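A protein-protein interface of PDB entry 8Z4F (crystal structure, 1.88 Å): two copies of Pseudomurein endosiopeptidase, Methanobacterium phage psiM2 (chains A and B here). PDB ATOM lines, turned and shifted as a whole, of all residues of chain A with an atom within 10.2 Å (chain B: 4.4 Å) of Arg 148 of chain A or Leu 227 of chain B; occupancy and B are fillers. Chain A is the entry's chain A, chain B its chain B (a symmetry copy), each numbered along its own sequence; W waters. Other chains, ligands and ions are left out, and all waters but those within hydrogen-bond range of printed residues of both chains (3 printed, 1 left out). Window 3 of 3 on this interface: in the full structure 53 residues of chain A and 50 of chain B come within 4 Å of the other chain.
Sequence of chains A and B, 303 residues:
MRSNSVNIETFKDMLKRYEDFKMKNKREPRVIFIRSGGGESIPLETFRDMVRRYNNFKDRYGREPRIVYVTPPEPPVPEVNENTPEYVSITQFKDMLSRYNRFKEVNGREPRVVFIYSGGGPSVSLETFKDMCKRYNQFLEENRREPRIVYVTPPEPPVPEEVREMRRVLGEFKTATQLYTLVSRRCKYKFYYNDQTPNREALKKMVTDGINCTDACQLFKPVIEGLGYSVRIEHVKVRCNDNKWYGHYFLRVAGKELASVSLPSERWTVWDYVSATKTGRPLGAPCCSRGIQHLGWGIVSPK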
ATOM      1  N   TYR A  87      28.305   3.559  -7.172  1.00  0.00           N
ATOM      2  CA  TYR A  87      27.613   2.383  -6.664  1.00  0.00           C
ATOM      3  C   TYR A  87      26.610   2.834  -5.621  1.00  0.00           C
ATOM      4  O   TYR A  87      26.675   3.959  -5.118  1.00  0.00           O
ATOM      5  CB  TYR A  87      28.573   1.354  -6.018  1.00  0.00           C
ATOM      6  CG  TYR A  87      29.447   2.008  -4.950  1.00  0.00           C
ATOM      7  CD1 TYR A  87      28.942   2.298  -3.680  1.00  0.00           C
ATOM      8  CD2 TYR A  87      30.755   2.363  -5.229  1.00  0.00           C
ATOM      9  CE1 TYR A  87      29.727   2.927  -2.712  1.00  0.00           C
ATOM     10  CE2 TYR A  87      31.554   3.009  -4.268  1.00  0.00           C
ATOM     11  CZ  TYR A  87      31.034   3.273  -3.010  1.00  0.00           C
ATOM     12  OH  TYR A  87      31.828   3.895  -2.053  1.00  0.00           O
ATOM     13  N   VAL A  88      25.694   1.929  -5.281  1.00  0.00           N
ATOM     14  CA  VAL A  88      24.770   2.111  -4.165  1.00  0.00           C
ATOM     15  C   VAL A  88      24.894   0.889  -3.267  1.00  0.00           C
ATOM     16  O   VAL A  88      25.235  -0.204  -3.722  1.00  0.00           O
ATOM     17  CB  VAL A  88      23.304   2.267  -4.615  1.00  0.00           C
ATOM     18  CG1 VAL A  88      23.112   3.524  -5.474  1.00  0.00           C
ATOM     19  CG2 VAL A  88      22.839   1.008  -5.402  1.00  0.00           C
ATOM     20  N   SER A  89      24.577   1.074  -1.994  1.00  0.00           N
ATOM     21  CA  SER A  89      24.454  -0.055  -1.088  1.00  0.00           C
ATOM     22  C   SER A  89      23.269  -0.937  -1.476  1.00  0.00           C
ATOM     23  O   SER A  89      22.345  -0.512  -2.194  1.00  0.00           O
ATOM     24  CB  SER A  89      24.264   0.460   0.330  1.00  0.00           C
ATOM     25  OG  SER A  89      23.002   1.104   0.406  1.00  0.00           O
ATOM     26  N   ILE A  90      23.285  -2.179  -0.974  1.00  0.00           N
ATOM     27  CA  ILE A  90      22.167  -3.097  -1.216  1.00  0.00           C
ATOM     28  C   ILE A  90      20.894  -2.521  -0.616  1.00  0.00           C
ATOM     29  O   ILE A  90      19.797  -2.680  -1.182  1.00  0.00           O
ATOM     30  CB  ILE A  90      22.470  -4.522  -0.667  1.00  0.00           C
ATOM     31  CG1 ILE A  90      21.363  -5.514  -1.035  1.00  0.00           C
ATOM     32  CG2 ILE A  90      22.686  -4.533   0.888  1.00  0.00           C
ATOM     33  CD1 ILE A  90      21.266  -5.789  -2.539  1.00  0.00           C
ATOM     34  N   THR A  91      21.014  -1.826   0.521  1.00  0.00           N
ATOM     35  CA  THR A  91      19.860  -1.190   1.138  1.00  0.00           C
ATOM     36  C   THR A  91      19.222  -0.211   0.161  1.00  0.00           C
ATOM     37  O   THR A  91      18.002  -0.235  -0.062  1.00  0.00           O
ATOM     38  CB  THR A  91      20.256  -0.429   2.405  1.00  0.00           C
ATOM     39  OG1 THR A  91      20.830  -1.318   3.369  1.00  0.00           O
ATOM     40  CG2 THR A  91      19.022   0.289   3.008  1.00  0.00           C
ATOM     41  N   GLN A  92      20.049   0.644  -0.440  1.00  0.00           N
ATOM     42  CA  GLN A  92      19.491   1.658  -1.330  1.00  0.00           C
ATOM     43  C   GLN A  92      19.020   1.033  -2.629  1.00  0.00           C
ATOM     44  O   GLN A  92      18.021   1.473  -3.196  1.00  0.00           O
ATOM     45  CB  GLN A  92      20.508   2.751  -1.635  1.00  0.00           C
ATOM     46  CG  GLN A  92      19.823   4.023  -2.199  1.00  0.00           C
ATOM     47  CD  GLN A  92      18.919   4.671  -1.156  1.00  0.00           C
ATOM     48  OE1 GLN A  92      19.245   4.670   0.050  1.00  0.00           O
ATOM     49  NE2 GLN A  92      17.776   5.208  -1.593  1.00  0.00           N
ATOM     50  N   PHE A  93      19.758   0.054  -3.156  1.00  0.00           N
ATOM     51  CA  PHE A  93      19.298  -0.613  -4.375  1.00  0.00           C
ATOM     52  C   PHE A  93      17.920  -1.231  -4.189  1.00  0.00           C
ATOM     53  O   PHE A  93      17.051  -1.121  -5.069  1.00  0.00           O
ATOM     54  CB  PHE A  93      20.309  -1.653  -4.853  1.00  0.00           C
ATOM     55  CG  PHE A  93      19.776  -2.508  -5.980  1.00  0.00           C
ATOM     56  CD1 PHE A  93      19.620  -1.980  -7.270  1.00  0.00           C
ATOM     57  CD2 PHE A  93      19.367  -3.805  -5.747  1.00  0.00           C
ATOM     58  CE1 PHE A  93      19.105  -2.773  -8.314  1.00  0.00           C
ATOM     59  CE2 PHE A  93      18.856  -4.597  -6.795  1.00  0.00           C
ATOM     60  CZ  PHE A  93      18.721  -4.057  -8.065  1.00  0.00           C
ATOM     61  N   LYS A  94      17.671  -1.857  -3.044  1.00  0.00           N
ATOM     62  CA  LYS A  94      16.366  -2.497  -2.897  1.00  0.00           C
ATOM     63  C   LYS A  94      15.273  -1.460  -2.738  1.00  0.00           C
ATOM     64  O   LYS A  94      14.125  -1.692  -3.137  1.00  0.00           O
ATOM     65  CB  LYS A  94      16.355  -3.467  -1.711  1.00  0.00           C
ATOM     66  CG  LYS A  94      17.354  -4.625  -1.860  1.00  0.00           C
ATOM     67  CD  LYS A  94      17.095  -5.491  -3.087  1.00  0.00           C
ATOM     68  CE  LYS A  94      15.875  -6.373  -2.875  1.00  0.00           C
ATOM     69  NZ  LYS A  94      16.161  -7.327  -1.764  1.00  0.00           N
ATOM     70  N   ARG A 135      23.022  -7.222 -13.305  1.00  0.00           N
ATOM     71  CA  ARG A 135      24.235  -7.604 -12.596  1.00  0.00           C
ATOM     72  C   ARG A 135      23.925  -8.020 -11.158  1.00  0.00           C
ATOM     73  O   ARG A 135      24.619  -8.878 -10.588  1.00  0.00           O
ATOM     74  CB  ARG A 135      25.244  -6.457 -12.639  1.00  0.00           C
ATOM     75  CG  ARG A 135      25.999  -6.347 -13.977  1.00  0.00           C
ATOM     76  CD  ARG A 135      26.981  -5.181 -14.030  1.00  0.00           C
ATOM     77  NE  ARG A 135      26.312  -3.895 -14.211  1.00  0.00           N
ATOM     78  CZ  ARG A 135      26.096  -3.035 -13.226  1.00  0.00           C
ATOM     79  NH1 ARG A 135      26.517  -3.268 -11.993  1.00  0.00           N
ATOM     80  NH2 ARG A 135      25.453  -1.908 -13.483  1.00  0.00           N
ATOM     81  N   TYR A 136      22.882  -7.442 -10.558  1.00  0.00           N
ATOM     82  CA  TYR A 136      22.440  -7.899  -9.246  1.00  0.00           C
ATOM     83  C   TYR A 136      21.951  -9.339  -9.321  1.00  0.00           C
ATOM     84  O   TYR A 136      22.256 -10.170  -8.455  1.00  0.00           O
ATOM     85  CB  TYR A 136      21.321  -7.006  -8.741  1.00  0.00           C
ATOM     86  CG  TYR A 136      20.508  -7.572  -7.586  1.00  0.00           C
ATOM     87  CD1 TYR A 136      21.000  -7.557  -6.279  1.00  0.00           C
ATOM     88  CD2 TYR A 136      19.248  -8.099  -7.803  1.00  0.00           C
ATOM     89  CE1 TYR A 136      20.235  -8.054  -5.224  1.00  0.00           C
ATOM     90  CE2 TYR A 136      18.480  -8.603  -6.767  1.00  0.00           C
ATOM     91  CZ  TYR A 136      18.979  -8.576  -5.486  1.00  0.00           C
ATOM     92  OH  TYR A 136      18.203  -9.075  -4.468  1.00  0.00           O
ATOM     93  N   PHE A 139      24.839 -11.743  -9.709  1.00  0.00           N
ATOM     94  CA  PHE A 139      25.556 -11.961  -8.455  1.00  0.00           C
ATOM     95  C   PHE A 139      24.796 -12.936  -7.575  1.00  0.00           C
ATOM     96  O   PHE A 139      25.389 -13.824  -6.957  1.00  0.00           O
ATOM     97  CB  PHE A 139      25.754 -10.626  -7.725  1.00  0.00           C
ATOM     98  CG  PHE A 139      26.606 -10.713  -6.488  1.00  0.00           C
ATOM     99  CD1 PHE A 139      26.103 -11.243  -5.300  1.00  0.00           C
ATOM    100  CD2 PHE A 139      27.902 -10.225  -6.498  1.00  0.00           C
ATOM    101  CE1 PHE A 139      26.879 -11.305  -4.165  1.00  0.00           C
ATOM    102  CE2 PHE A 139      28.684 -10.287  -5.357  1.00  0.00           C
ATOM    103  CZ  PHE A 139      28.163 -10.826  -4.189  1.00  0.00           C
ATOM    104  N   LEU A 140      23.479 -12.761  -7.492  1.00  0.00           N
ATOM    105  CA  LEU A 140      22.634 -13.692  -6.762  1.00  0.00           C
ATOM    106  C   LEU A 140      22.789 -15.115  -7.291  1.00  0.00           C
ATOM    107  O   LEU A 140      22.669 -16.073  -6.524  1.00  0.00           O
ATOM    108  CB  LEU A 140      21.183 -13.237  -6.875  1.00  0.00           C
ATOM    109  CG  LEU A 140      20.462 -12.558  -5.718  1.00  0.00           C
ATOM    110  CD1 LEU A 140      18.984 -12.797  -5.893  1.00  0.00           C
ATOM    111  CD2 LEU A 140      20.928 -13.086  -4.375  1.00  0.00           C
ATOM    112  N   ASN A 143      27.197 -16.252  -6.700  1.00  0.00           N
ATOM    113  CA  ASN A 143      27.179 -16.443  -5.263  1.00  0.00           C
ATOM    114  C   ASN A 143      25.767 -16.869  -4.883  1.00  0.00           C
ATOM    115  O   ASN A 143      24.913 -17.063  -5.745  1.00  0.00           O
ATOM    116  CB  ASN A 143      27.639 -15.164  -4.582  1.00  0.00           C
ATOM    117  CG  ASN A 143      28.763 -14.496  -5.349  1.00  0.00           C
ATOM    118  OD1 ASN A 143      29.918 -14.923  -5.297  1.00  0.00           O
ATOM    119  ND2 ASN A 143      28.414 -13.481  -6.133  1.00  0.00           N
ATOM    120  N   ARG A 145      23.884 -15.271  -2.326  1.00  0.00           N
ATOM    121  CA  ARG A 145      23.540 -14.248  -1.356  1.00  0.00           C
ATOM    122  C   ARG A 145      23.481 -12.908  -2.076  1.00  0.00           C
ATOM    123  O   ARG A 145      24.034 -12.743  -3.168  1.00  0.00           O
ATOM    124  CB  ARG A 145      24.569 -14.197  -0.223  1.00  0.00           C
ATOM    125  CG  ARG A 145      25.996 -14.302  -0.726  1.00  0.00           C
ATOM    126  CD  ARG A 145      27.016 -13.983   0.339  1.00  0.00           C
ATOM    127  NE  ARG A 145      27.612 -12.673   0.097  1.00  0.00           N
ATOM    128  CZ  ARG A 145      28.685 -12.464  -0.656  1.00  0.00           C
ATOM    129  NH1 ARG A 145      29.286 -13.459  -1.297  1.00  0.00           N
ATOM    130  NH2 ARG A 145      29.158 -11.224  -0.779  1.00  0.00           N
ATOM    131  N   GLU A 146      22.814 -11.948  -1.444  1.00  0.00           N
ATOM    132  CA  GLU A 146      22.768 -10.598  -1.989  1.00  0.00           C
ATOM    133  C   GLU A 146      24.139  -9.943  -1.859  1.00  0.00           C
ATOM    134  O   GLU A 146      24.851 -10.179  -0.882  1.00  0.00           O
ATOM    135  CB  GLU A 146      21.714  -9.759  -1.256  1.00  0.00           C
ATOM    136  CG  GLU A 146      20.295 -10.022  -1.728  1.00  0.00           C
ATOM    137  CD  GLU A 146      19.304  -8.988  -1.233  1.00  0.00           C
ATOM    138  OE1 GLU A 146      19.397  -8.583  -0.054  1.00  0.00           O
ATOM    139  OE2 GLU A 146      18.428  -8.571  -2.024  1.00  0.00           O
ATOM    140  N   PRO A 147      24.550  -9.138  -2.832  1.00  0.00           N
ATOM    141  CA  PRO A 147      25.799  -8.385  -2.684  1.00  0.00           C
ATOM    142  C   PRO A 147      25.595  -7.291  -1.654  1.00  0.00           C
ATOM    143  O   PRO A 147      24.462  -6.985  -1.283  1.00  0.00           O
ATOM    144  CB  PRO A 147      26.024  -7.801  -4.082  1.00  0.00           C
ATOM    145  CG  PRO A 147      24.595  -7.639  -4.628  1.00  0.00           C
ATOM    146  CD  PRO A 147      23.808  -8.776  -4.059  1.00  0.00           C
ATOM    147  N   ARG A 148      26.701  -6.713  -1.166  1.00  0.00           N
ATOM    148  CA  ARG A 148      26.571  -5.584  -0.244  1.00  0.00           C
ATOM    149  C   ARG A 148      26.465  -4.241  -0.968  1.00  0.00           C
ATOM    150  O   ARG A 148      25.914  -3.284  -0.406  1.00  0.00           O
ATOM    151  CB  ARG A 148      27.756  -5.545   0.721  1.00  0.00           C
ATOM    152  CG  ARG A 148      27.640  -6.611   1.823  1.00  0.00           C
ATOM    153  CD  ARG A 148      28.616  -6.419   2.956  1.00  0.00           C
ATOM    154  NE  ARG A 148      29.106  -7.709   3.439  1.00  0.00           N
ATOM    155  CZ  ARG A 148      30.190  -8.324   2.975  1.00  0.00           C
ATOM    156  NH1 ARG A 148      30.938  -7.784   2.023  1.00  0.00           N
ATOM    157  NH2 ARG A 148      30.529  -9.510   3.475  1.00  0.00           N
ATOM    158  N   ILE A 149      27.013  -4.143  -2.179  1.00  0.00           N
ATOM    159  CA  ILE A 149      26.862  -2.959  -3.019  1.00  0.00           C
ATOM    160  C   ILE A 149      26.484  -3.395  -4.430  1.00  0.00           C
ATOM    161  O   ILE A 149      26.720  -4.536  -4.843  1.00  0.00           O
ATOM    162  CB  ILE A 149      28.118  -2.055  -3.053  1.00  0.00           C
ATOM    163  CG1 ILE A 149      29.204  -2.633  -3.948  1.00  0.00           C
ATOM    164  CG2 ILE A 149      28.601  -1.635  -1.626  1.00  0.00           C
ATOM    165  CD1 ILE A 149      30.481  -1.852  -3.867  1.00  0.00           C
ATOM    166  N   VAL A 150      25.878  -2.464  -5.173  1.00  0.00           N
ATOM    167  CA  VAL A 150      25.484  -2.697  -6.564  1.00  0.00           C
ATOM    168  C   VAL A 150      26.037  -1.510  -7.349  1.00  0.00           C
ATOM    169  O   VAL A 150      25.698  -0.353  -7.041  1.00  0.00           O
ATOM    170  CB  VAL A 150      23.954  -2.789  -6.723  1.00  0.00           C
ATOM    171  CG1 VAL A 150      23.548  -2.810  -8.212  1.00  0.00           C
ATOM    172  CG2 VAL A 150      23.361  -4.005  -5.964  1.00  0.00           C
ATOM    173  N   TYR A 151      26.917  -1.779  -8.318  1.00  0.00           N
ATOM    174  CA  TYR A 151      27.533  -0.695  -9.070  1.00  0.00           C
ATOM    175  C   TYR A 151      26.519  -0.093 -10.035  1.00  0.00           C
ATOM    176  O   TYR A 151      25.821  -0.828 -10.740  1.00  0.00           O
ATOM    177  CB  TYR A 151      28.736  -1.186  -9.852  1.00  0.00           C
ATOM    178  CG  TYR A 151      29.949  -1.324  -8.968  1.00  0.00           C
ATOM    179  CD1 TYR A 151      30.716  -0.227  -8.644  1.00  0.00           C
ATOM    180  CD2 TYR A 151      30.289  -2.551  -8.431  1.00  0.00           C
ATOM    181  CE1 TYR A 151      31.827  -0.346  -7.799  1.00  0.00           C
ATOM    182  CE2 TYR A 151      31.393  -2.691  -7.608  1.00  0.00           C
ATOM    183  CZ  TYR A 151      32.148  -1.586  -7.296  1.00  0.00           C
ATOM    184  OH  TYR A 151      33.246  -1.728  -6.471  1.00  0.00           O
ATOM    185  N   ARG B 167      39.351  -1.339   8.761  1.00  0.00           N
ATOM    186  CA  ARG B 167      39.410  -2.436   9.713  1.00  0.00           C
ATOM    187  C   ARG B 167      40.822  -2.594  10.245  1.00  0.00           C
ATOM    188  O   ARG B 167      41.017  -2.810  11.446  1.00  0.00           O
ATOM    189  CB  ARG B 167      38.918  -3.738   9.071  1.00  0.00           C
ATOM    190  CG  ARG B 167      37.387  -3.791   8.912  1.00  0.00           C
ATOM    191  CD  ARG B 167      36.912  -5.041   8.203  1.00  0.00           C
ATOM    192  NE  ARG B 167      35.459  -5.207   8.271  1.00  0.00           N
ATOM    193  CZ  ARG B 167      34.755  -5.916   7.398  1.00  0.00           C
ATOM    194  NH1 ARG B 167      35.341  -6.566   6.409  1.00  0.00           N
ATOM    195  NH2 ARG B 167      33.432  -5.978   7.524  1.00  0.00           N
ATOM    196  N   PHE B 173      34.869  -4.856  12.431  1.00  0.00           N
ATOM    197  CA  PHE B 173      33.503  -4.394  12.608  1.00  0.00           C
ATOM    198  C   PHE B 173      32.709  -4.857  11.395  1.00  0.00           C
ATOM    199  O   PHE B 173      33.256  -4.979  10.293  1.00  0.00           O
ATOM    200  CB  PHE B 173      33.456  -2.875  12.762  1.00  0.00           C
ATOM    201  CG  PHE B 173      34.090  -2.148  11.606  1.00  0.00           C
ATOM    202  CD1 PHE B 173      33.350  -1.866  10.465  1.00  0.00           C
ATOM    203  CD2 PHE B 173      35.425  -1.774  11.655  1.00  0.00           C
ATOM    204  CE1 PHE B 173      33.942  -1.218   9.382  1.00  0.00           C
ATOM    205  CE2 PHE B 173      36.029  -1.122  10.587  1.00  0.00           C
ATOM    206  CZ  PHE B 173      35.286  -0.845   9.441  1.00  0.00           C
ATOM    207  N   LYS B 174      31.426  -5.151  11.622  1.00  0.00           N
ATOM    208  CA  LYS B 174      30.497  -5.501  10.558  1.00  0.00           C
ATOM    209  C   LYS B 174      29.241  -4.634  10.509  1.00  0.00           C
ATOM    210  O   LYS B 174      28.521  -4.722   9.508  1.00  0.00           O
ATOM    211  CB  LYS B 174      30.053  -6.972  10.689  1.00  0.00           C
ATOM    212  CG  LYS B 174      31.208  -7.951  10.840  1.00  0.00           C
ATOM    213  CD  LYS B 174      30.715  -9.398  10.920  1.00  0.00           C
ATOM    214  CE  LYS B 174      29.810  -9.587  12.156  1.00  0.00           C
ATOM    215  NZ  LYS B 174      30.448  -9.223  13.475  1.00  0.00           N
ATOM    216  N   THR B 175      28.936  -3.840  11.551  1.00  0.00           N
ATOM    217  CA  THR B 175      27.738  -3.008  11.607  1.00  0.00           C
ATOM    218  C   THR B 175      28.112  -1.536  11.799  1.00  0.00           C
ATOM    219  O   THR B 175      29.216  -1.206  12.261  1.00  0.00           O
ATOM    220  CB  THR B 175      26.781  -3.430  12.754  1.00  0.00           C
ATOM    221  OG1 THR B 175      27.388  -3.099  14.031  1.00  0.00           O
ATOM    222  CG2 THR B 175      26.450  -4.933  12.700  1.00  0.00           C
ATOM    223  N   ALA B 176      27.181  -0.637  11.445  1.00  0.00           N
ATOM    224  CA  ALA B 176      27.431   0.794  11.672  1.00  0.00           C
ATOM    225  C   ALA B 176      27.477   1.119  13.170  1.00  0.00           C
ATOM    226  O   ALA B 176      28.178   2.055  13.582  1.00  0.00           O
ATOM    227  CB  ALA B 176      26.356   1.650  10.977  1.00  0.00           C
ATOM    228  N   VAL B 223      32.771   3.372   3.649  1.00  0.00           N
ATOM    229  CA  VAL B 223      32.902   2.199   4.516  1.00  0.00           C
ATOM    230  C   VAL B 223      31.528   1.711   4.948  1.00  0.00           C
ATOM    231  O   VAL B 223      31.237   0.511   4.912  1.00  0.00           O
ATOM    232  CB  VAL B 223      33.774   2.522   5.746  1.00  0.00           C
ATOM    233  CG1 VAL B 223      33.741   1.350   6.735  1.00  0.00           C
ATOM    234  CG2 VAL B 223      35.222   2.846   5.336  1.00  0.00           C
ATOM    235  N   ILE B 224      30.679   2.634   5.403  1.00  0.00           N
ATOM    236  CA  ILE B 224      29.350   2.259   5.879  1.00  0.00           C
ATOM    237  C   ILE B 224      28.468   1.790   4.726  1.00  0.00           C
ATOM    238  O   ILE B 224      27.671   0.853   4.877  1.00  0.00           O
ATOM    239  CB  ILE B 224      28.730   3.427   6.663  1.00  0.00           C
ATOM    240  CG1 ILE B 224      29.543   3.667   7.957  1.00  0.00           C
ATOM    241  CG2 ILE B 224      27.266   3.161   6.967  1.00  0.00           C
ATOM    242  CD1 ILE B 224      29.235   4.965   8.648  1.00  0.00           C
ATOM    243  N   GLU B 225      28.607   2.397   3.547  1.00  0.00           N
ATOM    244  CA  GLU B 225      27.912   1.821   2.388  1.00  0.00           C
ATOM    245  C   GLU B 225      28.421   0.422   2.077  1.00  0.00           C
ATOM    246  O   GLU B 225      27.634  -0.475   1.749  1.00  0.00           O
ATOM    247  CB  GLU B 225      28.076   2.732   1.172  1.00  0.00           C
ATOM    248  CG  GLU B 225      27.178   3.903   1.258  1.00  0.00           C
ATOM    249  CD  GLU B 225      27.209   4.732  -0.017  1.00  0.00           C
ATOM    250  OE1 GLU B 225      28.310   5.109  -0.473  1.00  0.00           O
ATOM    251  OE2 GLU B 225      26.128   4.982  -0.549  1.00  0.00           O
ATOM    252  N   GLY B 226      29.735   0.210   2.177  1.00  0.00           N
ATOM    253  CA  GLY B 226      30.310  -1.098   1.912  1.00  0.00           C
ATOM    254  C   GLY B 226      29.902  -2.165   2.910  1.00  0.00           C
ATOM    255  O   GLY B 226      29.958  -3.365   2.587  1.00  0.00           O
ATOM    256  N   LEU B 227      29.467  -1.762   4.098  1.00  0.00           N
ATOM    257  CA  LEU B 227      28.799  -2.692   4.998  1.00  0.00           C
ATOM    258  C   LEU B 227      27.375  -2.998   4.567  1.00  0.00           C
ATOM    259  O   LEU B 227      26.758  -3.893   5.143  1.00  0.00           O
ATOM    260  CB  LEU B 227      28.764  -2.139   6.429  1.00  0.00           C
ATOM    261  CG  LEU B 227      30.141  -1.842   7.035  1.00  0.00           C
ATOM    262  CD1 LEU B 227      30.032  -1.334   8.495  1.00  0.00           C
ATOM    263  CD2 LEU B 227      31.054  -3.066   6.919  1.00  0.00           C
ATOM    264  N   GLY B 228      26.811  -2.258   3.606  1.00  0.00           N
ATOM    265  CA  GLY B 228      25.455  -2.523   3.155  1.00  0.00           C
ATOM    266  C   GLY B 228      24.398  -1.490   3.530  1.00  0.00           C
ATOM    267  O   GLY B 228      23.240  -1.661   3.120  1.00  0.00           O
ATOM    268  N   TYR B 229      24.752  -0.424   4.260  1.00  0.00           N
ATOM    269  CA  TYR B 229      23.818   0.624   4.675  1.00  0.00           C
ATOM    270  C   TYR B 229      23.632   1.677   3.578  1.00  0.00           C
ATOM    271  O   TYR B 229      24.570   1.998   2.850  1.00  0.00           O
ATOM    272  CB  TYR B 229      24.330   1.359   5.918  1.00  0.00           C
ATOM    273  CG  TYR B 229      24.486   0.466   7.099  1.00  0.00           C
ATOM    274  CD1 TYR B 229      25.622  -0.328   7.231  1.00  0.00           C
ATOM    275  CD2 TYR B 229      23.487   0.379   8.051  1.00  0.00           C
ATOM    276  CE1 TYR B 229      25.784  -1.182   8.321  1.00  0.00           C
ATOM    277  CE2 TYR B 229      23.650  -0.480   9.182  1.00  0.00           C
ATOM    278  CZ  TYR B 229      24.783  -1.257   9.269  1.00  0.00           C
ATOM    279  OH  TYR B 229      24.944  -2.103  10.341  1.00  0.00           O
ATOM    280  N   LYS B 256      19.586  -2.274   7.646  1.00  0.00           N
ATOM    281  CA  LYS B 256      19.937  -3.189   8.734  1.00  0.00           C
ATOM    282  C   LYS B 256      19.366  -2.733  10.080  1.00  0.00           C
ATOM    283  O   LYS B 256      18.153  -2.514  10.190  1.00  0.00           O
ATOM    284  CB  LYS B 256      21.450  -3.374   8.752  1.00  0.00           C
ATOM    285  CG  LYS B 256      21.905  -3.852   7.350  1.00  0.00           C
ATOM    286  CD  LYS B 256      23.386  -3.674   7.098  1.00  0.00           C
ATOM    287  CE  LYS B 256      24.210  -4.462   8.096  1.00  0.00           C
ATOM    288  NZ  LYS B 256      24.327  -5.883   7.661  1.00  0.00           N
HETATM  289  O   HOH W   1      30.957   6.389  -1.434  1.00  0.00           O
HETATM  290  O   HOH W   2      26.364   5.753  -2.923  1.00  0.00           O
HETATM  291  O   HOH W   3      18.666  -3.139   5.267  1.00  0.00           O
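No position is printed for both chains.
Of the 13 pairs that touch across the chains among the printed residues, none has its exchanged pair printed and touching as well.
Among the printed residues, pairs that only touch across the chains: Tyr 87 of chain A with Glu 225 of chain B (3.4 Å), Ser 89 of chain A with Glu 225 of chain B (3.8 Å), Ser 89 of chain A with Gly 228 of chain B (3.7 Å), Ile 90 of chain A with Gly 228 of chain B (3.7 Å), Thr 91 of chain A with Tyr 229 of chain B (3.8 Å), Arg 148 of chain A with Glu 225 of chain B (3.9 Å), Arg 148 of chain A with Gly 226 of chain B (3.4 Å), Arg 148 of chain A with Leu 227 of chain B (3.8 Å), Arg 148 of chain A with Gly 228 of chain B (3.7 Å), Ile 149 of chain A with Glu 225 of chain B (3.7 Å) and Ile 149 of chain A with Gly 226 of chain B (3.97 Å).
Hydrophobic or aromatic side chains of chain A that line the printed part of chain B: Tyr 87, Ile 90 and Ile 149.
Printed residues of chain B that touch a printed residue of chain A: Glu 225, Gly 226, Leu 227, Gly 228 and Tyr 229.
Among the printed residues, no Asp or Glu carboxylate lies within 4 Å of a Lys or Arg side-chain nitrogen of the other chain.
The side-chain hydroxyl (OG) of Ser 89 of chain A sits at hydrogen-bond distance from the backbone NH (N) of Gln 92 of chain A, at 3.1 Å.
The backbone carbonyl oxygen (O) of Arg 148 of chain A sits at hydrogen-bond distance from the backbone NH (N) of Ile 90 of chain A (2.9 Å).
OH of Tyr 229 of chain B is in hydrogen-bond range of N of Ala 176 of chain B, at 2.9 Å.
The backbone carbonyl oxygen (O) of Ile 224 of chain B sits at hydrogen-bond distance from the backbone NH (N) of Tyr 229 of chain B, 3.2 Å away.
Water W2 lies within hydrogen-bond range of the side-chain carboxylate (OE2) of Glu 225 of chain B and the backbone carbonyl oxygen (O) of Tyr 87 of chain A.
Water W3 lies within hydrogen-bond range of N of Lys 256 of chain B (2.7 Å) and OG1 of Thr 91 of chain A (3.4 Å).
Water W1 bridges OH of Tyr 87 of chain A (2.7 Å) and OE1 of Glu 225 of chain B (3.1 Å).
OG of Ser 89 of chain A sits close to O of Tyr 229 of chain B, at 3.0 Å.
The backbone carbonyl oxygen (O) of Gly 228 of chain B is in hydrogen-bond range of the side-chain hydroxyl (OG1) of Thr 91 of chain A (2.4 Å).
Of chain B, only Glu 225, Gly 226, Leu 227 and Gly 228 come within 4 Å of Arg 148 of chain A.
Leu 227 of chain B touches just one residue of chain A: Arg 148 (3.8 Å).
Of chain A, only Arg 148 (3.4 Å) and Ile 149 (3.97 Å) come within 4 Å of Gly 226 of chain B.
Tyr 229 of chain B touches just these residues of chain A: Ser 89 and Thr 91.
Printed residues of chain B within 4 Å of Ile 90 of chain A: Gly 228.
Of the printed residues of chain B, Ser 89 of chain A touches Glu 225, Gly 228 and Tyr 229.
Of the printed residues of chain B, Ile 149 of chain A touches Glu 225 and Gly 226.
The nearest residue of chain A that does not touch Leu 227 of chain B is Ile 149 of chain A (5.8 Å).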
